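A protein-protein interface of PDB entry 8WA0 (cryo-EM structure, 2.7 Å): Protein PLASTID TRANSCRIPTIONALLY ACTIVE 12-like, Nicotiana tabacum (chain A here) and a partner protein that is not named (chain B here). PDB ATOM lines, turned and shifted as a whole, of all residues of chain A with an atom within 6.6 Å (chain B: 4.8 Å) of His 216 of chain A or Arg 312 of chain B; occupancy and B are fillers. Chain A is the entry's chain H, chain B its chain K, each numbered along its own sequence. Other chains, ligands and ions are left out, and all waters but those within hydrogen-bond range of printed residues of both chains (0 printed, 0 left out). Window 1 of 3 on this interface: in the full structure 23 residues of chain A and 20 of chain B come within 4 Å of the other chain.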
ATOM      1  N   GLY A 205      16.756  18.108  23.046  1.00  0.00           N
ATOM      2  CA  GLY A 205      16.423  16.749  22.794  1.00  0.00           C
ATOM      3  C   GLY A 205      17.666  15.922  22.749  1.00  0.00           C
ATOM      4  O   GLY A 205      17.681  14.853  23.333  1.00  0.00           O
ATOM      5  N   TYR A 206      18.719  16.377  22.108  1.00  0.00           N
ATOM      6  CA  TYR A 206      19.864  15.517  22.007  1.00  0.00           C
ATOM      7  C   TYR A 206      20.448  15.241  23.343  1.00  0.00           C
ATOM      8  O   TYR A 206      20.735  14.093  23.669  1.00  0.00           O
ATOM      9  CB  TYR A 206      20.934  16.093  21.121  1.00  0.00           C
ATOM     10  CG  TYR A 206      22.056  15.156  20.805  1.00  0.00           C
ATOM     11  CD1 TYR A 206      21.931  14.228  19.800  1.00  0.00           C
ATOM     12  CD2 TYR A 206      23.249  15.219  21.494  1.00  0.00           C
ATOM     13  CE1 TYR A 206      22.959  13.374  19.499  1.00  0.00           C
ATOM     14  CE2 TYR A 206      24.282  14.367  21.201  1.00  0.00           C
ATOM     15  CZ  TYR A 206      24.129  13.448  20.201  1.00  0.00           C
ATOM     16  OH  TYR A 206      25.158  12.593  19.902  1.00  0.00           O
ATOM     17  N   ASP A 209      18.153  12.977  25.487  1.00  0.00           N
ATOM     18  CA  ASP A 209      18.147  11.630  24.995  1.00  0.00           C
ATOM     19  C   ASP A 209      19.387  10.904  25.291  1.00  0.00           C
ATOM     20  O   ASP A 209      19.342   9.753  25.677  1.00  0.00           O
ATOM     21  CB  ASP A 209      17.852  11.609  23.532  1.00  0.00           C
ATOM     22  CG  ASP A 209      16.393  11.801  23.236  1.00  0.00           C
ATOM     23  OD1 ASP A 209      15.626  12.045  24.187  1.00  0.00           O
ATOM     24  OD2 ASP A 209      16.009  11.707  22.054  1.00  0.00           O
ATOM     25  N   LYS A 210      20.508  11.554  25.150  1.00  0.00           N
ATOM     26  CA  LYS A 210      21.752  10.950  25.477  1.00  0.00           C
ATOM     27  C   LYS A 210      21.885  10.606  26.924  1.00  0.00           C
ATOM     28  O   LYS A 210      22.354   9.532  27.243  1.00  0.00           O
ATOM     29  CB  LYS A 210      22.882  11.839  25.034  1.00  0.00           C
ATOM     30  CG  LYS A 210      24.232  11.174  24.940  1.00  0.00           C
ATOM     31  CD  LYS A 210      25.259  12.139  24.388  1.00  0.00           C
ATOM     32  CE  LYS A 210      26.621  11.485  24.285  1.00  0.00           C
ATOM     33  NZ  LYS A 210      27.120  11.056  25.619  1.00  0.00           N
ATOM     34  N   ARG A 211      21.470  11.464  27.827  1.00  0.00           N
ATOM     35  CA  ARG A 211      21.500  11.114  29.224  1.00  0.00           C
ATOM     36  C   ARG A 211      20.589   9.992  29.620  1.00  0.00           C
ATOM     37  O   ARG A 211      21.010   9.073  30.296  1.00  0.00           O
ATOM     38  CB  ARG A 211      21.118  12.305  30.065  1.00  0.00           C
ATOM     39  CG  ARG A 211      22.219  13.318  30.288  1.00  0.00           C
ATOM     40  CD  ARG A 211      21.765  14.420  31.232  1.00  0.00           C
ATOM     41  NE  ARG A 211      21.330  13.903  32.530  1.00  0.00           N
ATOM     42  CZ  ARG A 211      20.063  13.826  32.928  1.00  0.00           C
ATOM     43  NH1 ARG A 211      19.771  13.337  34.125  1.00  0.00           N
ATOM     44  NH2 ARG A 211      19.086  14.242  32.130  1.00  0.00           N
ATOM     45  N   GLY A 213      19.213   7.672  27.616  1.00  0.00           N
ATOM     46  CA  GLY A 213      19.518   6.458  26.917  1.00  0.00           C
ATOM     47  C   GLY A 213      18.603   6.132  25.791  1.00  0.00           C
ATOM     48  O   GLY A 213      18.716   5.074  25.212  1.00  0.00           O
ATOM     49  N   ARG A 214      17.697   7.014  25.454  1.00  0.00           N
ATOM     50  CA  ARG A 214      16.721   6.750  24.432  1.00  0.00           C
ATOM     51  C   ARG A 214      17.361   6.790  23.075  1.00  0.00           C
ATOM     52  O   ARG A 214      18.466   7.260  22.938  1.00  0.00           O
ATOM     53  CB  ARG A 214      15.591   7.765  24.554  1.00  0.00           C
ATOM     54  CG  ARG A 214      15.254   8.170  25.966  1.00  0.00           C
ATOM     55  CD  ARG A 214      14.135   9.188  25.957  1.00  0.00           C
ATOM     56  NE  ARG A 214      13.009   8.720  25.161  1.00  0.00           N
ATOM     57  CZ  ARG A 214      11.998   8.002  25.640  1.00  0.00           C
ATOM     58  NH1 ARG A 214      11.965   7.665  26.923  1.00  0.00           N
ATOM     59  NH2 ARG A 214      11.016   7.620  24.835  1.00  0.00           N
ATOM     60  N   PRO A 215      16.703   6.274  22.057  1.00  0.00           N
ATOM     61  CA  PRO A 215      17.374   6.257  20.774  1.00  0.00           C
ATOM     62  C   PRO A 215      17.803   7.601  20.255  1.00  0.00           C
ATOM     63  O   PRO A 215      16.997   8.501  20.233  1.00  0.00           O
ATOM     64  CB  PRO A 215      16.299   5.713  19.884  1.00  0.00           C
ATOM     65  CG  PRO A 215      15.556   4.759  20.726  1.00  0.00           C
ATOM     66  CD  PRO A 215      15.517   5.403  22.070  1.00  0.00           C
ATOM     67  N   HIS A 216      19.034   7.742  19.809  1.00  0.00           N
ATOM     68  CA  HIS A 216      19.578   8.998  19.315  1.00  0.00           C
ATOM     69  C   HIS A 216      20.734   8.826  18.347  1.00  0.00           C
ATOM     70  O   HIS A 216      21.389   7.805  18.366  1.00  0.00           O
ATOM     71  CB  HIS A 216      20.061   9.836  20.480  1.00  0.00           C
ATOM     72  CG  HIS A 216      21.350   9.406  21.078  1.00  0.00           C
ATOM     73  ND1 HIS A 216      21.420   8.426  22.035  1.00  0.00           N
ATOM     74  CD2 HIS A 216      22.609   9.866  20.912  1.00  0.00           C
ATOM     75  CE1 HIS A 216      22.675   8.266  22.395  1.00  0.00           C
ATOM     76  NE2 HIS A 216      23.416   9.130  21.734  1.00  0.00           N
ATOM     77  N   PRO A 217      21.016   9.809  17.508  1.00  0.00           N
ATOM     78  CA  PRO A 217      22.151   9.753  16.601  1.00  0.00           C
ATOM     79  C   PRO A 217      23.485   9.810  17.293  1.00  0.00           C
ATOM     80  O   PRO A 217      23.628  10.653  18.148  1.00  0.00           O
ATOM     81  CB  PRO A 217      21.983  11.004  15.792  1.00  0.00           C
ATOM     82  CG  PRO A 217      20.962  11.839  16.455  1.00  0.00           C
ATOM     83  CD  PRO A 217      20.075  10.870  17.135  1.00  0.00           C
ATOM     84  N   PHE A 218      24.474   9.009  16.953  1.00  0.00           N
ATOM     85  CA  PHE A 218      25.730   9.008  17.687  1.00  0.00           C
ATOM     86  C   PHE A 218      26.513  10.293  17.606  1.00  0.00           C
ATOM     87  O   PHE A 218      27.040  10.731  18.615  1.00  0.00           O
ATOM     88  CB  PHE A 218      26.645   7.923  17.175  1.00  0.00           C
ATOM     89  CG  PHE A 218      26.610   6.639  17.931  1.00  0.00           C
ATOM     90  CD1 PHE A 218      26.896   6.593  19.270  1.00  0.00           C
ATOM     91  CD2 PHE A 218      26.374   5.458  17.265  1.00  0.00           C
ATOM     92  CE1 PHE A 218      26.891   5.395  19.946  1.00  0.00           C
ATOM     93  CE2 PHE A 218      26.364   4.258  17.928  1.00  0.00           C
ATOM     94  CZ  PHE A 218      26.629   4.227  19.270  1.00  0.00           C
ATOM     95  N   ILE A 219      26.615  10.913  16.440  1.00  0.00           N
ATOM     96  CA  ILE A 219      27.297  12.200  16.254  1.00  0.00           C
ATOM     97  C   ILE A 219      26.236  13.282  16.177  1.00  0.00           C
ATOM     98  O   ILE A 219      25.308  13.159  15.399  1.00  0.00           O
ATOM     99  CB  ILE A 219      28.084  12.204  14.960  1.00  0.00           C
ATOM    100  CG1 ILE A 219      29.204  11.169  15.015  1.00  0.00           C
ATOM    101  CG2 ILE A 219      28.657  13.578  14.670  1.00  0.00           C
ATOM    102  CD1 ILE A 219      30.225  11.426  16.099  1.00  0.00           C
ATOM    103  N   LYS A 273      14.559   3.131  16.825  1.00  0.00           N
ATOM    104  CA  LYS A 273      14.594   3.978  15.661  1.00  0.00           C
ATOM    105  C   LYS A 273      16.002   3.935  15.210  1.00  0.00           C
ATOM    106  O   LYS A 273      16.890   4.014  16.013  1.00  0.00           O
ATOM    107  CB  LYS A 273      14.188   5.396  15.987  1.00  0.00           C
ATOM    108  CG  LYS A 273      12.753   5.549  16.431  1.00  0.00           C
ATOM    109  CD  LYS A 273      12.423   7.003  16.702  1.00  0.00           C
ATOM    110  CE  LYS A 273      10.991   7.152  17.185  1.00  0.00           C
ATOM    111  NZ  LYS A 273      10.023   6.561  16.220  1.00  0.00           N
ATOM    112  N   TRP B 308      26.462   1.860  34.663  1.00  0.00           N
ATOM    113  CA  TRP B 308      25.909   2.323  33.425  1.00  0.00           C
ATOM    114  C   TRP B 308      26.722   3.380  32.752  1.00  0.00           C
ATOM    115  O   TRP B 308      26.900   3.319  31.545  1.00  0.00           O
ATOM    116  CB  TRP B 308      24.503   2.834  33.602  1.00  0.00           C
ATOM    117  CG  TRP B 308      23.569   2.655  32.456  1.00  0.00           C
ATOM    118  CD1 TRP B 308      22.718   1.623  32.262  1.00  0.00           C
ATOM    119  CD2 TRP B 308      23.360   3.553  31.368  1.00  0.00           C
ATOM    120  NE1 TRP B 308      22.005   1.805  31.119  1.00  0.00           N
ATOM    121  CE2 TRP B 308      22.386   2.984  30.545  1.00  0.00           C
ATOM    122  CE3 TRP B 308      23.914   4.775  31.003  1.00  0.00           C
ATOM    123  CZ2 TRP B 308      21.954   3.590  29.387  1.00  0.00           C
ATOM    124  CZ3 TRP B 308      23.487   5.370  29.861  1.00  0.00           C
ATOM    125  CH2 TRP B 308      22.516   4.784  29.062  1.00  0.00           C
ATOM    126  N   LYS B 309      27.258   4.328  33.463  1.00  0.00           N
ATOM    127  CA  LYS B 309      28.103   5.313  32.856  1.00  0.00           C
ATOM    128  C   LYS B 309      29.345   4.789  32.270  1.00  0.00           C
ATOM    129  O   LYS B 309      29.668   5.105  31.143  1.00  0.00           O
ATOM    130  CB  LYS B 309      28.472   6.330  33.904  1.00  0.00           C
ATOM    131  CG  LYS B 309      29.152   7.576  33.382  1.00  0.00           C
ATOM    132  CD  LYS B 309      29.777   8.357  34.523  1.00  0.00           C
ATOM    133  CE  LYS B 309      30.825   7.521  35.242  1.00  0.00           C
ATOM    134  NZ  LYS B 309      31.933   7.118  34.330  1.00  0.00           N
ATOM    135  N   LYS B 310      30.047   3.952  32.978  1.00  0.00           N
ATOM    136  CA  LYS B 310      31.264   3.376  32.491  1.00  0.00           C
ATOM    137  C   LYS B 310      31.077   2.465  31.328  1.00  0.00           C
ATOM    138  O   LYS B 310      31.806   2.556  30.365  1.00  0.00           O
ATOM    139  CB  LYS B 310      31.937   2.643  33.616  1.00  0.00           C
ATOM    140  CG  LYS B 310      32.257   3.504  34.818  1.00  0.00           C
ATOM    141  CD  LYS B 310      33.222   2.795  35.754  1.00  0.00           C
ATOM    142  CE  LYS B 310      32.712   1.419  36.152  1.00  0.00           C
ATOM    143  NZ  LYS B 310      31.499   1.492  37.010  1.00  0.00           N
ATOM    144  N   SER B 311      30.077   1.617  31.373  1.00  0.00           N
ATOM    145  CA  SER B 311      29.773   0.720  30.309  1.00  0.00           C
ATOM    146  C   SER B 311      29.396   1.444  29.046  1.00  0.00           C
ATOM    147  O   SER B 311      29.786   1.018  27.979  1.00  0.00           O
ATOM    148  CB  SER B 311      28.671  -0.187  30.755  1.00  0.00           C
ATOM    149  OG  SER B 311      27.525   0.535  31.126  1.00  0.00           O
ATOM    150  N   ARG B 312      28.639   2.529  29.123  1.00  0.00           N
ATOM    151  CA  ARG B 312      28.316   3.270  27.945  1.00  0.00           C
ATOM    152  C   ARG B 312      29.474   3.899  27.268  1.00  0.00           C
ATOM    153  O   ARG B 312      29.629   3.757  26.067  1.00  0.00           O
ATOM    154  CB  ARG B 312      27.231   4.287  28.164  1.00  0.00           C
ATOM    155  CG  ARG B 312      26.065   4.151  27.227  1.00  0.00           C
ATOM    156  CD  ARG B 312      25.688   5.480  26.629  1.00  0.00           C
ATOM    157  NE  ARG B 312      26.347   5.695  25.359  1.00  0.00           N
ATOM    158  CZ  ARG B 312      25.864   6.474  24.411  1.00  0.00           C
ATOM    159  NH1 ARG B 312      24.717   7.094  24.597  1.00  0.00           N
ATOM    160  NH2 ARG B 312      26.517   6.629  23.279  1.00  0.00           N
ATOM    161  N   GLN B 313      30.333   4.533  27.996  1.00  0.00           N
ATOM    162  CA  GLN B 313      31.483   5.116  27.426  1.00  0.00           C
ATOM    163  C   GLN B 313      32.392   4.099  26.792  1.00  0.00           C
ATOM    164  O   GLN B 313      32.940   4.349  25.726  1.00  0.00           O
ATOM    165  CB  GLN B 313      32.196   5.911  28.473  1.00  0.00           C
ATOM    166  CG  GLN B 313      31.383   7.069  29.014  1.00  0.00           C
ATOM    167  CD  GLN B 313      31.001   8.074  27.943  1.00  0.00           C
ATOM    168  OE1 GLN B 313      29.854   8.516  27.875  1.00  0.00           O
ATOM    169  NE2 GLN B 313      31.960   8.439  27.098  1.00  0.00           N
ATOM    170  N   ASP B 314      32.563   2.954  27.392  1.00  0.00           N
ATOM    171  CA  ASP B 314      33.360   1.905  26.825  1.00  0.00           C
ATOM    172  C   ASP B 314      32.870   1.305  25.531  1.00  0.00           C
ATOM    173  O   ASP B 314      33.674   1.042  24.653  1.00  0.00           O
ATOM    174  CB  ASP B 314      33.560   0.856  27.854  1.00  0.00           C
ATOM    175  CG  ASP B 314      34.489   1.294  28.950  1.00  0.00           C
ATOM    176  OD1 ASP B 314      35.194   2.305  28.761  1.00  0.00           O
ATOM    177  OD2 ASP B 314      34.520   0.629  30.005  1.00  0.00           O
ATOM    178  N   MET B 315      31.587   1.088  25.357  1.00  0.00           N
ATOM    179  CA  MET B 315      31.048   0.618  24.104  1.00  0.00           C
ATOM    180  C   MET B 315      31.247   1.585  22.978  1.00  0.00           C
ATOM    181  O   MET B 315      31.532   1.172  21.868  1.00  0.00           O
ATOM    182  CB  MET B 315      29.598   0.251  24.208  1.00  0.00           C
ATOM    183  CG  MET B 315      29.014  -0.506  23.038  1.00  0.00           C
ATOM    184  SD  MET B 315      29.399  -2.255  23.107  1.00  0.00           S
ATOM    185  CE  MET B 315      28.642  -2.846  21.598  1.00  0.00           C
ATOM    186  N   GLU B 316      31.104   2.864  23.218  1.00  0.00           N
ATOM    187  CA  GLU B 316      31.347   3.836  22.198  1.00  0.00           C
ATOM    188  C   GLU B 316      32.758   3.821  21.741  1.00  0.00           C
ATOM    189  O   GLU B 316      33.018   3.954  20.553  1.00  0.00           O
ATOM    190  CB  GLU B 316      31.006   5.244  22.616  1.00  0.00           C
ATOM    191  CG  GLU B 316      29.725   5.407  23.396  1.00  0.00           C
ATOM    192  CD  GLU B 316      29.730   6.684  24.213  1.00  0.00           C
ATOM    193  OE1 GLU B 316      29.038   6.738  25.251  1.00  0.00           O
ATOM    194  OE2 GLU B 316      30.446   7.630  23.826  1.00  0.00           O
ATOM    195  N   SER B 328      25.333   5.949  12.224  1.00  0.00           N
ATOM    196  CA  SER B 328      24.593   5.032  13.083  1.00  0.00           C
ATOM    197  C   SER B 328      23.829   5.661  14.250  1.00  0.00           C
ATOM    198  O   SER B 328      24.026   6.821  14.524  1.00  0.00           O
ATOM    199  CB  SER B 328      25.569   4.019  13.596  1.00  0.00           C
ATOM    200  OG  SER B 328      26.339   3.486  12.561  1.00  0.00           O
ATOM    201  N   ASN B 329      22.960   4.920  14.940  1.00  0.00           N
ATOM    202  CA  ASN B 329      22.153   5.427  16.032  1.00  0.00           C
ATOM    203  C   ASN B 329      22.235   4.547  17.264  1.00  0.00           C
ATOM    204  O   ASN B 329      22.132   3.344  17.124  1.00  0.00           O
ATOM    205  CB  ASN B 329      20.717   5.460  15.503  1.00  0.00           C
ATOM    206  CG  ASN B 329      19.801   6.384  16.224  1.00  0.00           C
ATOM    207  OD1 ASN B 329      19.338   6.089  17.319  1.00  0.00           O
ATOM    208  ND2 ASN B 329      19.455   7.480  15.576  1.00  0.00           N
ATOM    209  N   TRP B 330      22.434   5.085  18.465  1.00  0.00           N
ATOM    210  CA  TRP B 330      22.365   4.287  19.683  1.00  0.00           C
ATOM    211  C   TRP B 330      20.943   3.941  19.933  1.00  0.00           C
ATOM    212  O   TRP B 330      20.087   4.780  19.788  1.00  0.00           O
ATOM    213  CB  TRP B 330      22.808   5.037  20.898  1.00  0.00           C
ATOM    214  CG  TRP B 330      23.395   4.160  21.954  1.00  0.00           C
ATOM    215  CD1 TRP B 330      24.575   3.481  21.891  1.00  0.00           C
ATOM    216  CD2 TRP B 330      22.839   3.868  23.232  1.00  0.00           C
ATOM    217  NE1 TRP B 330      24.785   2.778  23.051  1.00  0.00           N
ATOM    218  CE2 TRP B 330      23.730   3.000  23.890  1.00  0.00           C
ATOM    219  CE3 TRP B 330      21.676   4.248  23.881  1.00  0.00           C
ATOM    220  CZ2 TRP B 330      23.492   2.512  25.152  1.00  0.00           C
ATOM    221  CZ3 TRP B 330      21.444   3.762  25.135  1.00  0.00           C
ATOM    222  CH2 TRP B 330      22.345   2.907  25.763  1.00  0.00           C
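The guanidinium group of Arg 312 of chain B lies within salt-bridge range of the side-chain carboxylate of Glu 316 of chain B (2.9 Å). The backbone carbonyl oxygen (O) of Pro 217 of chain A is in hydrogen-bond range of the side-chain hydroxyl (OH) of Tyr 206 of chain A, at 3.0 Å. The side-chain hydroxyl (OH) of Tyr 206 of chain A lies within hydrogen-bond range of the backbone carbonyl oxygen (O) of Phe 218 of chain A, 2.9 Å away. O of Arg 214 of chain A sits at hydrogen-bond distance from ND1 of His 216 of chain A, at 3.3 Å.
The backbone carbonyl oxygen (O) of Ser 328 of chain B is in hydrogen-bond range of the backbone NH (N) of Phe 218 of chain A. The backbone carbonyl oxygen (O) of His 216 of chain A lies close to the side-chain amide oxygen (OD1) of Asn 329 of chain B (2.9 Å). O of Lys 273 of chain A lies close to OD1 of Asn 329 of chain B. The backbone carbonyl oxygen of His 216 of chain A sits at hydrogen-bond distance from the backbone NH of Trp 330 of chain B. N of Pro 217 of chain A sits close to ND2 of Asn 329 of chain B (3.4 Å).
Asp 209 of chain A touches none of the printed residues of chain B. Of the printed residues of chain B, Gly 213 of chain A touches Trp 330 (3.0 Å). His 216 of chain A touches just these residues of chain B: Arg 312 (3.2 Å), Asn 329 (2.9 Å) and Trp 330 (2.9 Å). Printed residues of chain B within 4 Å of Phe 218 of chain A: Arg 312 (3.6 Å), Ser 328 (3.3 Å) and Trp 330 (3.4 Å). Trp 308 of chain B touches none of the printed residues of chain A. Of chain A, only His 216 and Phe 218 come within 4 Å of Arg 312 of chain B. The nearest residue of chain A that does not touch Arg 312 of chain B is Lys 210 of chain A (4.1 Å).
Among the printed residues, merely in contact across the chains: Gly 213 of chain A with Trp 330 of chain B (3.0 Å), His 216 of chain A with Arg 312 of chain B (3.2 Å), Pro 215 of chain A with Trp 330 of chain B (3.2 Å), Phe 218 of chain A with Trp 330 of chain B (3.4 Å), Phe 218 of chain A with Arg 312 of chain B (3.6 Å) and Pro 215 of chain A with Asn 329 of chain B (3.6 Å).
Of the 13 printed residues of chain A, 6 touch a printed residue of chain B. Along chain A the printed residues that touch a printed residue of chain B span positions 213 to 273. Of the 12 printed residues of chain B, 4 touch a printed residue of chain A.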
